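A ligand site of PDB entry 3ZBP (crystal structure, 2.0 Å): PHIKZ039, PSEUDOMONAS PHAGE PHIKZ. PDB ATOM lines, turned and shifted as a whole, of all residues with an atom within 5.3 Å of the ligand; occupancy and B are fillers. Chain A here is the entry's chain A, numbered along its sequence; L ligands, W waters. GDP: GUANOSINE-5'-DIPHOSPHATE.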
ATOM      1  N   CYS A  12      14.474  20.475  24.464  1.00  0.00           N
ATOM      2  CA  CYS A  12      13.417  21.452  24.737  1.00  0.00           C
ATOM      3  C   CYS A  12      12.191  20.841  25.423  1.00  0.00           C
ATOM      4  O   CYS A  12      11.708  19.790  25.019  1.00  0.00           O
ATOM      5  CB  CYS A  12      12.964  22.135  23.433  1.00  0.00           C
ATOM      6  SG  CYS A  12      14.308  22.756  22.395  1.00  0.00           S
ATOM      7  N   GLY A  13      11.682  21.523  26.449  1.00  0.00           N
ATOM      8  CA  GLY A  13      10.480  21.065  27.130  1.00  0.00           C
ATOM      9  C   GLY A  13      10.783  19.864  28.010  1.00  0.00           C
ATOM     10  O   GLY A  13      11.944  19.467  28.136  1.00  0.00           O
ATOM     11  N   GLY A  14       9.745  19.275  28.602  1.00  0.00           N
ATOM     12  CA  GLY A  14       9.899  18.167  29.537  1.00  0.00           C
ATOM     13  C   GLY A  14      10.551  16.937  28.947  1.00  0.00           C
ATOM     14  O   GLY A  14      11.507  16.413  29.517  1.00  0.00           O
ATOM     15  N   ALA A  15      10.028  16.438  27.825  1.00  0.00           N
ATOM     16  CA  ALA A  15      10.579  15.239  27.195  1.00  0.00           C
ATOM     17  C   ALA A  15      12.031  15.474  26.832  1.00  0.00           C
ATOM     18  O   ALA A  15      12.880  14.588  27.010  1.00  0.00           O
ATOM     19  CB  ALA A  15       9.751  14.854  25.954  1.00  0.00           C
ATOM     20  N   GLY A  16      12.316  16.669  26.325  1.00  0.00           N
ATOM     21  CA  GLY A  16      13.668  17.052  25.974  1.00  0.00           C
ATOM     22  C   GLY A  16      14.621  17.010  27.143  1.00  0.00           C
ATOM     23  O   GLY A  16      15.756  16.518  27.022  1.00  0.00           O
ATOM     24  N   ARG A  18      14.261  15.227  29.940  1.00  0.00           N
ATOM     25  CA  ARG A  18      14.406  13.826  30.335  1.00  0.00           C
ATOM     26  C   ARG A  18      15.388  13.081  29.412  1.00  0.00           C
ATOM     27  O   ARG A  18      16.254  12.336  29.881  1.00  0.00           O
ATOM     28  CB  ARG A  18      13.034  13.141  30.357  1.00  0.00           C
ATOM     29  CG  ARG A  18      12.109  13.645  31.477  1.00  0.00           C
ATOM     30  CD  ARG A  18      10.595  13.658  31.132  1.00  0.00           C
ATOM     31  NE  ARG A  18       9.886  14.486  32.112  1.00  0.00           N
ATOM     32  CZ  ARG A  18       8.828  15.274  31.848  1.00  0.00           C
ATOM     33  NH1 ARG A  18       8.307  15.337  30.628  1.00  0.00           N
ATOM     34  NH2 ARG A  18       8.295  15.988  32.824  1.00  0.00           N
ATOM     35  N   ILE A  19      15.266  13.295  28.111  1.00  0.00           N
ATOM     36  CA  ILE A  19      16.183  12.663  27.157  1.00  0.00           C
ATOM     37  C   ILE A  19      17.608  13.173  27.345  1.00  0.00           C
ATOM     38  O   ILE A  19      18.572  12.393  27.353  1.00  0.00           O
ATOM     39  CB  ILE A  19      15.701  12.863  25.704  1.00  0.00           C
ATOM     40  CG1 ILE A  19      14.379  12.117  25.509  1.00  0.00           C
ATOM     41  CG2 ILE A  19      16.744  12.332  24.706  1.00  0.00           C
ATOM     42  CD1 ILE A  19      13.584  12.539  24.276  1.00  0.00           C
ATOM     43  N   ASP A  34      13.442  25.633  28.467  1.00  0.00           N
ATOM     44  CA  ASP A  34      12.101  25.309  28.966  1.00  0.00           C
ATOM     45  C   ASP A  34      11.373  26.560  29.426  1.00  0.00           C
ATOM     46  O   ASP A  34      11.957  27.660  29.480  1.00  0.00           O
ATOM     47  CB  ASP A  34      12.193  24.299  30.107  1.00  0.00           C
ATOM     48  CG  ASP A  34      10.951  23.420  30.217  1.00  0.00           C
ATOM     49  OD1 ASP A  34       9.940  23.665  29.522  1.00  0.00           O
ATOM     50  OD2 ASP A  34      10.978  22.462  31.033  1.00  0.00           O
ATOM     51  N   ASN A  39      11.131  20.973  35.324  1.00  0.00           N
ATOM     52  CA  ASN A  39      11.746  19.802  34.683  1.00  0.00           C
ATOM     53  C   ASN A  39      13.253  19.685  34.903  1.00  0.00           C
ATOM     54  O   ASN A  39      13.893  18.739  34.423  1.00  0.00           O
ATOM     55  CB  ASN A  39      11.440  19.802  33.200  1.00  0.00           C
ATOM     56  CG  ASN A  39       9.970  19.527  32.918  1.00  0.00           C
ATOM     57  OD1 ASN A  39       9.391  18.601  33.471  1.00  0.00           O
ATOM     58  ND2 ASN A  39       9.355  20.357  32.066  1.00  0.00           N
ATOM     59  N   ILE A  68      -0.281  27.126  30.179  1.00  0.00           N
ATOM     60  CA  ILE A  68       0.910  26.650  29.470  1.00  0.00           C
ATOM     61  C   ILE A  68       1.392  25.315  30.046  1.00  0.00           C
ATOM     62  O   ILE A  68       1.632  24.362  29.300  1.00  0.00           O
ATOM     63  CB  ILE A  68       2.066  27.681  29.520  1.00  0.00           C
ATOM     64  CG1 ILE A  68       1.699  28.949  28.722  1.00  0.00           C
ATOM     65  CG2 ILE A  68       3.364  27.062  28.983  1.00  0.00           C
ATOM     66  CD1 ILE A  68       2.626  30.146  28.993  1.00  0.00           C
ATOM     67  N   LYS A  72      -1.289  22.781  28.602  1.00  0.00           N
ATOM     68  CA  LYS A  72      -0.470  22.612  27.398  1.00  0.00           C
ATOM     69  C   LYS A  72      -1.027  23.412  26.223  1.00  0.00           C
ATOM     70  O   LYS A  72      -1.088  22.920  25.101  1.00  0.00           O
ATOM     71  CB  LYS A  72      -0.310  21.138  27.020  1.00  0.00           C
ATOM     72  CG  LYS A  72       0.262  20.247  28.130  1.00  0.00           C
ATOM     73  CD  LYS A  72       1.672  20.641  28.533  1.00  0.00           C
ATOM     74  CE  LYS A  72       2.251  19.619  29.519  1.00  0.00           C
ATOM     75  NZ  LYS A  72       3.422  20.194  30.259  1.00  0.00           N
ATOM     76  N   SER A 103       8.970  16.804  22.502  1.00  0.00           N
ATOM     77  CA  SER A 103       7.701  16.113  22.273  1.00  0.00           C
ATOM     78  C   SER A 103       6.813  17.011  21.435  1.00  0.00           C
ATOM     79  O   SER A 103       6.965  18.233  21.468  1.00  0.00           O
ATOM     80  CB  SER A 103       7.003  15.810  23.586  1.00  0.00           C
ATOM     81  OG  SER A 103       6.639  17.020  24.252  1.00  0.00           O
ATOM     82  N   GLY A 105       3.424  16.613  21.801  1.00  0.00           N
ATOM     83  CA  GLY A 105       2.147  16.616  22.506  1.00  0.00           C
ATOM     84  C   GLY A 105       2.030  17.612  23.647  1.00  0.00           C
ATOM     85  O   GLY A 105       0.934  17.836  24.175  1.00  0.00           O
ATOM     86  N   GLY A 106       3.152  18.232  24.022  1.00  0.00           N
ATOM     87  CA  GLY A 106       3.124  19.236  25.073  1.00  0.00           C
ATOM     88  C   GLY A 106       3.071  20.635  24.476  1.00  0.00           C
ATOM     89  O   GLY A 106       2.699  20.809  23.302  1.00  0.00           O
ATOM     90  N   ALA A 107       3.436  21.633  25.268  1.00  0.00           N
ATOM     91  CA  ALA A 107       3.340  23.004  24.804  1.00  0.00           C
ATOM     92  C   ALA A 107       4.676  23.726  24.727  1.00  0.00           C
ATOM     93  O   ALA A 107       4.834  24.684  23.956  1.00  0.00           O
ATOM     94  CB  ALA A 107       2.360  23.792  25.669  1.00  0.00           C
ATOM     95  N   SER A 108       5.638  23.305  25.542  1.00  0.00           N
ATOM     96  CA  SER A 108       6.929  24.000  25.566  1.00  0.00           C
ATOM     97  C   SER A 108       7.873  23.510  24.473  1.00  0.00           C
ATOM     98  O   SER A 108       8.386  24.303  23.671  1.00  0.00           O
ATOM     99  CB  SER A 108       7.567  23.889  26.949  1.00  0.00           C
ATOM    100  OG  SER A 108       6.770  24.602  27.890  1.00  0.00           O
ATOM    101  N   GLY A 109       8.117  22.203  24.429  1.00  0.00           N
ATOM    102  CA  GLY A 109       8.982  21.668  23.405  1.00  0.00           C
ATOM    103  C   GLY A 109       8.414  21.892  22.024  1.00  0.00           C
ATOM    104  O   GLY A 109       9.143  22.189  21.080  1.00  0.00           O
ATOM    105  N   SER A 110       7.090  21.794  21.899  1.00  0.00           N
ATOM    106  CA  SER A 110       6.436  21.781  20.588  1.00  0.00           C
ATOM    107  C   SER A 110       6.304  23.179  20.023  1.00  0.00           C
ATOM    108  O   SER A 110       5.835  23.349  18.898  1.00  0.00           O
ATOM    109  CB  SER A 110       5.061  21.130  20.671  1.00  0.00           C
ATOM    110  OG  SER A 110       4.155  21.954  21.391  1.00  0.00           O
ATOM    111  N   ILE A 132       8.580  13.457  19.307  1.00  0.00           N
ATOM    112  CA  ILE A 132       7.729  12.393  19.849  1.00  0.00           C
ATOM    113  C   ILE A 132       6.253  12.724  19.686  1.00  0.00           C
ATOM    114  O   ILE A 132       5.774  13.733  20.232  1.00  0.00           O
ATOM    115  CB  ILE A 132       7.979  12.200  21.376  1.00  0.00           C
ATOM    116  CG1 ILE A 132       9.427  11.804  21.659  1.00  0.00           C
ATOM    117  CG2 ILE A 132       7.020  11.137  21.940  1.00  0.00           C
ATOM    118  CD1 ILE A 132       9.864  12.075  23.114  1.00  0.00           C
ATOM    119  N   SER A 134       2.284  11.725  20.478  1.00  0.00           N
ATOM    120  CA  SER A 134       1.584  11.016  21.535  1.00  0.00           C
ATOM    121  C   SER A 134       0.090  11.223  21.489  1.00  0.00           C
ATOM    122  O   SER A 134      -0.420  12.118  20.803  1.00  0.00           O
ATOM    123  CB  SER A 134       2.122  11.431  22.909  1.00  0.00           C
ATOM    124  OG  SER A 134       1.983  12.824  23.078  1.00  0.00           O
ATOM    125  N   ASP A 136      -1.854  10.080  24.626  1.00  0.00           N
ATOM    126  CA  ASP A 136      -2.265   9.617  25.958  1.00  0.00           C
ATOM    127  C   ASP A 136      -3.451  10.395  26.522  1.00  0.00           C
ATOM    128  O   ASP A 136      -4.037   9.996  27.531  1.00  0.00           O
ATOM    129  CB  ASP A 136      -1.090   9.648  26.963  1.00  0.00           C
ATOM    130  CG  ASP A 136      -0.414  11.013  27.036  1.00  0.00           C
ATOM    131  OD1 ASP A 136       0.475  11.287  26.199  1.00  0.00           O
ATOM    132  OD2 ASP A 136      -0.742  11.806  27.932  1.00  0.00           O
ATOM    133  N   SER A 140      -2.882  15.789  24.316  1.00  0.00           N
ATOM    134  CA  SER A 140      -1.695  15.282  23.625  1.00  0.00           C
ATOM    135  C   SER A 140      -1.964  15.051  22.141  1.00  0.00           C
ATOM    136  O   SER A 140      -1.135  15.403  21.287  1.00  0.00           O
ATOM    137  CB  SER A 140      -1.233  13.965  24.267  1.00  0.00           C
ATOM    138  OG  SER A 140      -0.780  14.210  25.581  1.00  0.00           O
ATOM    139  N   ASN A 169       4.809   7.534  20.948  1.00  0.00           N
ATOM    140  CA  ASN A 169       4.481   6.898  22.228  1.00  0.00           C
ATOM    141  C   ASN A 169       3.342   5.905  22.057  1.00  0.00           C
ATOM    142  O   ASN A 169       2.180   6.222  22.344  1.00  0.00           O
ATOM    143  CB  ASN A 169       4.100   7.948  23.266  1.00  0.00           C
ATOM    144  CG  ASN A 169       5.310   8.594  23.927  1.00  0.00           C
ATOM    145  OD1 ASN A 169       6.455   8.164  23.725  1.00  0.00           O
ATOM    146  ND2 ASN A 169       5.060   9.637  24.725  1.00  0.00           N
ATOM    147  N   GLN A 175       7.651   4.848  28.158  1.00  0.00           N
ATOM    148  CA  GLN A 175       8.353   5.982  27.591  1.00  0.00           C
ATOM    149  C   GLN A 175       9.865   5.811  27.669  1.00  0.00           C
ATOM    150  O   GLN A 175      10.612   6.358  26.849  1.00  0.00           O
ATOM    151  CB  GLN A 175       7.903   7.280  28.275  1.00  0.00           C
ATOM    152  CG  GLN A 175       6.428   7.557  28.036  1.00  0.00           C
ATOM    153  CD  GLN A 175       5.997   8.914  28.537  1.00  0.00           C
ATOM    154  OE1 GLN A 175       6.772   9.607  29.208  1.00  0.00           O
ATOM    155  NE2 GLN A 175       4.772   9.307  28.207  1.00  0.00           N
ATOM    156  N   VAL A 178      10.958   4.203  24.417  1.00  0.00           N
ATOM    157  CA  VAL A 178      11.004   5.232  23.376  1.00  0.00           C
ATOM    158  C   VAL A 178      12.248   6.106  23.571  1.00  0.00           C
ATOM    159  O   VAL A 178      12.979   6.359  22.618  1.00  0.00           O
ATOM    160  CB  VAL A 178       9.731   6.094  23.366  1.00  0.00           C
ATOM    161  CG1 VAL A 178       9.856   7.251  22.359  1.00  0.00           C
ATOM    162  CG2 VAL A 178       8.516   5.241  23.043  1.00  0.00           C
ATOM    163  N   ASN A 179      12.510   6.537  24.797  1.00  0.00           N
ATOM    164  CA  ASN A 179      13.682   7.343  25.097  1.00  0.00           C
ATOM    165  C   ASN A 179      14.985   6.646  24.708  1.00  0.00           C
ATOM    166  O   ASN A 179      15.890   7.256  24.141  1.00  0.00           O
ATOM    167  CB  ASN A 179      13.701   7.708  26.585  1.00  0.00           C
ATOM    168  CG  ASN A 179      12.691   8.773  26.931  1.00  0.00           C
ATOM    169  OD1 ASN A 179      11.931   9.220  26.071  1.00  0.00           O
ATOM    170  ND2 ASN A 179      12.670   9.189  28.193  1.00  0.00           N
ATOM    171  N   ILE A 182      15.495   6.854  21.104  1.00  0.00           N
ATOM    172  CA  ILE A 182      15.934   8.212  20.759  1.00  0.00           C
ATOM    173  C   ILE A 182      17.428   8.380  21.034  1.00  0.00           C
ATOM    174  O   ILE A 182      18.136   9.051  20.274  1.00  0.00           O
ATOM    175  CB  ILE A 182      15.105   9.264  21.521  1.00  0.00           C
ATOM    176  CG1 ILE A 182      13.692   9.282  20.938  1.00  0.00           C
ATOM    177  CG2 ILE A 182      15.756  10.641  21.432  1.00  0.00           C
ATOM    178  CD1 ILE A 182      12.669  10.121  21.720  1.00  0.00           C
HETATM  179  PB  GDP L   1       6.178  20.173  27.529  1.00  0.00           P
HETATM  180  O1B GDP L   1       5.073  21.203  27.633  1.00  0.00           O
HETATM  181  O2B GDP L   1       7.183  20.336  28.637  1.00  0.00           O
HETATM  182  O3B GDP L   1       6.875  20.368  26.208  1.00  0.00           O
HETATM  183  O3A GDP L   1       5.442  18.723  27.552  1.00  0.00           O
HETATM  184  PA  GDP L   1       6.163  17.305  27.809  1.00  0.00           P
HETATM  185  O1A GDP L   1       7.398  17.136  26.982  1.00  0.00           O
HETATM  186  O2A GDP L   1       6.529  17.141  29.260  1.00  0.00           O
HETATM  187  O5' GDP L   1       4.982  16.244  27.534  1.00  0.00           O
HETATM  188  C5' GDP L   1       4.210  16.181  26.338  1.00  0.00           C
HETATM  189  C4' GDP L   1       3.942  14.740  25.899  1.00  0.00           C
HETATM  190  O4' GDP L   1       5.185  14.042  25.906  1.00  0.00           O
HETATM  191  C3' GDP L   1       3.008  13.933  26.793  1.00  0.00           C
HETATM  192  O3' GDP L   1       2.295  13.034  25.930  1.00  0.00           O
HETATM  193  C2' GDP L   1       3.939  13.083  27.633  1.00  0.00           C
HETATM  194  O2' GDP L   1       3.316  11.854  27.976  1.00  0.00           O
HETATM  195  C1' GDP L   1       5.100  12.848  26.682  1.00  0.00           C
HETATM  196  N9  GDP L   1       6.405  12.732  27.368  1.00  0.00           N
HETATM  197  C8  GDP L   1       6.809  13.508  28.379  1.00  0.00           C
HETATM  198  N7  GDP L   1       8.058  13.169  28.763  1.00  0.00           N
HETATM  199  C5  GDP L   1       8.478  12.165  27.968  1.00  0.00           C
HETATM  200  C6  GDP L   1       9.702  11.368  27.845  1.00  0.00           C
HETATM  201  O6  GDP L   1      10.673  11.570  28.624  1.00  0.00           O
HETATM  202  N1  GDP L   1       9.752  10.419  26.893  1.00  0.00           N
HETATM  203  C2  GDP L   1       8.706  10.204  26.066  1.00  0.00           C
HETATM  204  N2  GDP L   1       8.822   9.228  25.127  1.00  0.00           N
HETATM  205  N3  GDP L   1       7.546  10.901  26.135  1.00  0.00           N
HETATM  206  C4  GDP L   1       7.383  11.886  27.041  1.00  0.00           C
HETATM  207  O   HOH W   1       2.254   9.547  25.587  1.00  0.00           O
HETATM  208  O   HOH W   2       6.492  19.445  31.200  1.00  0.00           O
HETATM  209  O   HOH W   3       9.022   9.411  30.807  1.00  0.00           O
HETATM  210  O   HOH W   4       4.542  23.337  28.901  1.00  0.00           O
HETATM  211  O   HOH W   5       5.889  19.876  23.811  1.00  0.00           O
HETATM  212  O   HOH W   6       7.640  22.390  30.167  1.00  0.00           O
HETATM  213  O   HOH W   7       4.367  17.451  30.915  1.00  0.00           O
HETATM  214  O   HOH W   8       4.137  14.071  22.520  1.00  0.00           O
HETATM  215  O   HOH W   9       9.404  18.361  24.972  1.00  0.00           O
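OD1 of Asp 136 sits at hydrogen-bond distance from O3' of the ligand (2.5 Å). A nitrogen (N1) of the ligand lies within hydrogen-bond range of the side-chain amide oxygen (OD1) of Asn 179, at 2.6 Å. O2B of the ligand sits at hydrogen-bond distance from N of Gly 14 (2.8 Å). The side-chain hydroxyl (OG) of Ser 103 is in hydrogen-bond range of an oxygen (O1A) of the ligand, at 2.8 Å. The backbone NH (N) of Gly 109 lies within hydrogen-bond range of an oxygen (O3B) of the ligand, 2.8 Å away. The backbone NH (N) of Ala 15 is in hydrogen-bond range of an oxygen (O1A) of the ligand (2.8 Å). The guanidinium group (NH1) of Arg 18 lies within salt-bridge range of an oxygen (O2A) of the ligand (2.9 Å). O3' of the ligand is in hydrogen-bond range of OG of Ser 134, at 2.9 Å. An oxygen (O1B) of the ligand sits at hydrogen-bond distance from the backbone NH (N) of Ala 107 (2.9 Å). O2' of the ligand is in hydrogen-bond range of NE2 of Gln 175 (2.9 Å). The side-chain amide oxygen (OD1) of Asn 169 sits at hydrogen-bond distance from a nitrogen (N2) of the ligand, at 2.9 Å. N of Ser 108 lies within hydrogen-bond range of O1B of the ligand (3.0 Å). The side-chain amino group of Lys 72 is in salt-bridge range of an oxygen (O1B) of the ligand, 3.3 Å away. OG of Ser 140 is in hydrogen-bond range of O3' of the ligand, at 3.3 Å.
OD1 of Asp 136 sits at hydrogen-bond distance from OG of Ser 140. OD1 of Asn 179 sits close to O of Gln 175. NH2 of Arg 18 sits at hydrogen-bond distance from OD1 of Asn 39, 2.9 Å away. The backbone carbonyl oxygen of Gly 106 lies within hydrogen-bond range of the side-chain hydroxyl of Ser 110, 2.7 Å away.
Merely in contact with the ligand: Gly 13, Gly 105, Gly 106, Ile 132 and Val 178. Hydrophobic or aromatic side chains that line the ligand: Ala 15, Ile 132 and Val 178. Of the 27 residues printed, 19 come within 4 Å of the ligand. Along chain A the residues within 4 Å of the ligand span positions 13 to 179. The nearest printed residue that does not touch the ligand is Asn 39 (4.1 Å).
Water W4 lies within hydrogen-bond range of O1B of the ligand (2.5 Å), OG of Ser 108 (2.8 Å) and O of Ile 68 (3.1 Å). Water W7 lies within hydrogen-bond range of O2A of the ligand (2.7 Å) and NZ of Lys 72 (3.0 Å). Water W9 lies within hydrogen-bond range of the backbone carbonyl oxygen of Cys 12 (2.7 Å), the backbone NH of Ser 103 (3.0 Å), an oxygen (O1A) of the ligand (3.1 Å) and the backbone NH of Ala 15 (3.5 Å). Water W8 lies within hydrogen-bond range of OG of Ser 134 (2.6 Å), N of Gly 105 (2.7 Å) and O of Ile 132 (2.8 Å). Water W3 bridges OE1 of Gln 175 (2.8 Å) and O6 of the ligand (3.5 Å). Water W1 lies within hydrogen-bond range of the side-chain carboxylate of Asp 136 (2.6 Å), the side-chain amide nitrogen of Asn 169 (2.9 Å) and an oxygen (O2') of the ligand (3.5 Å).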
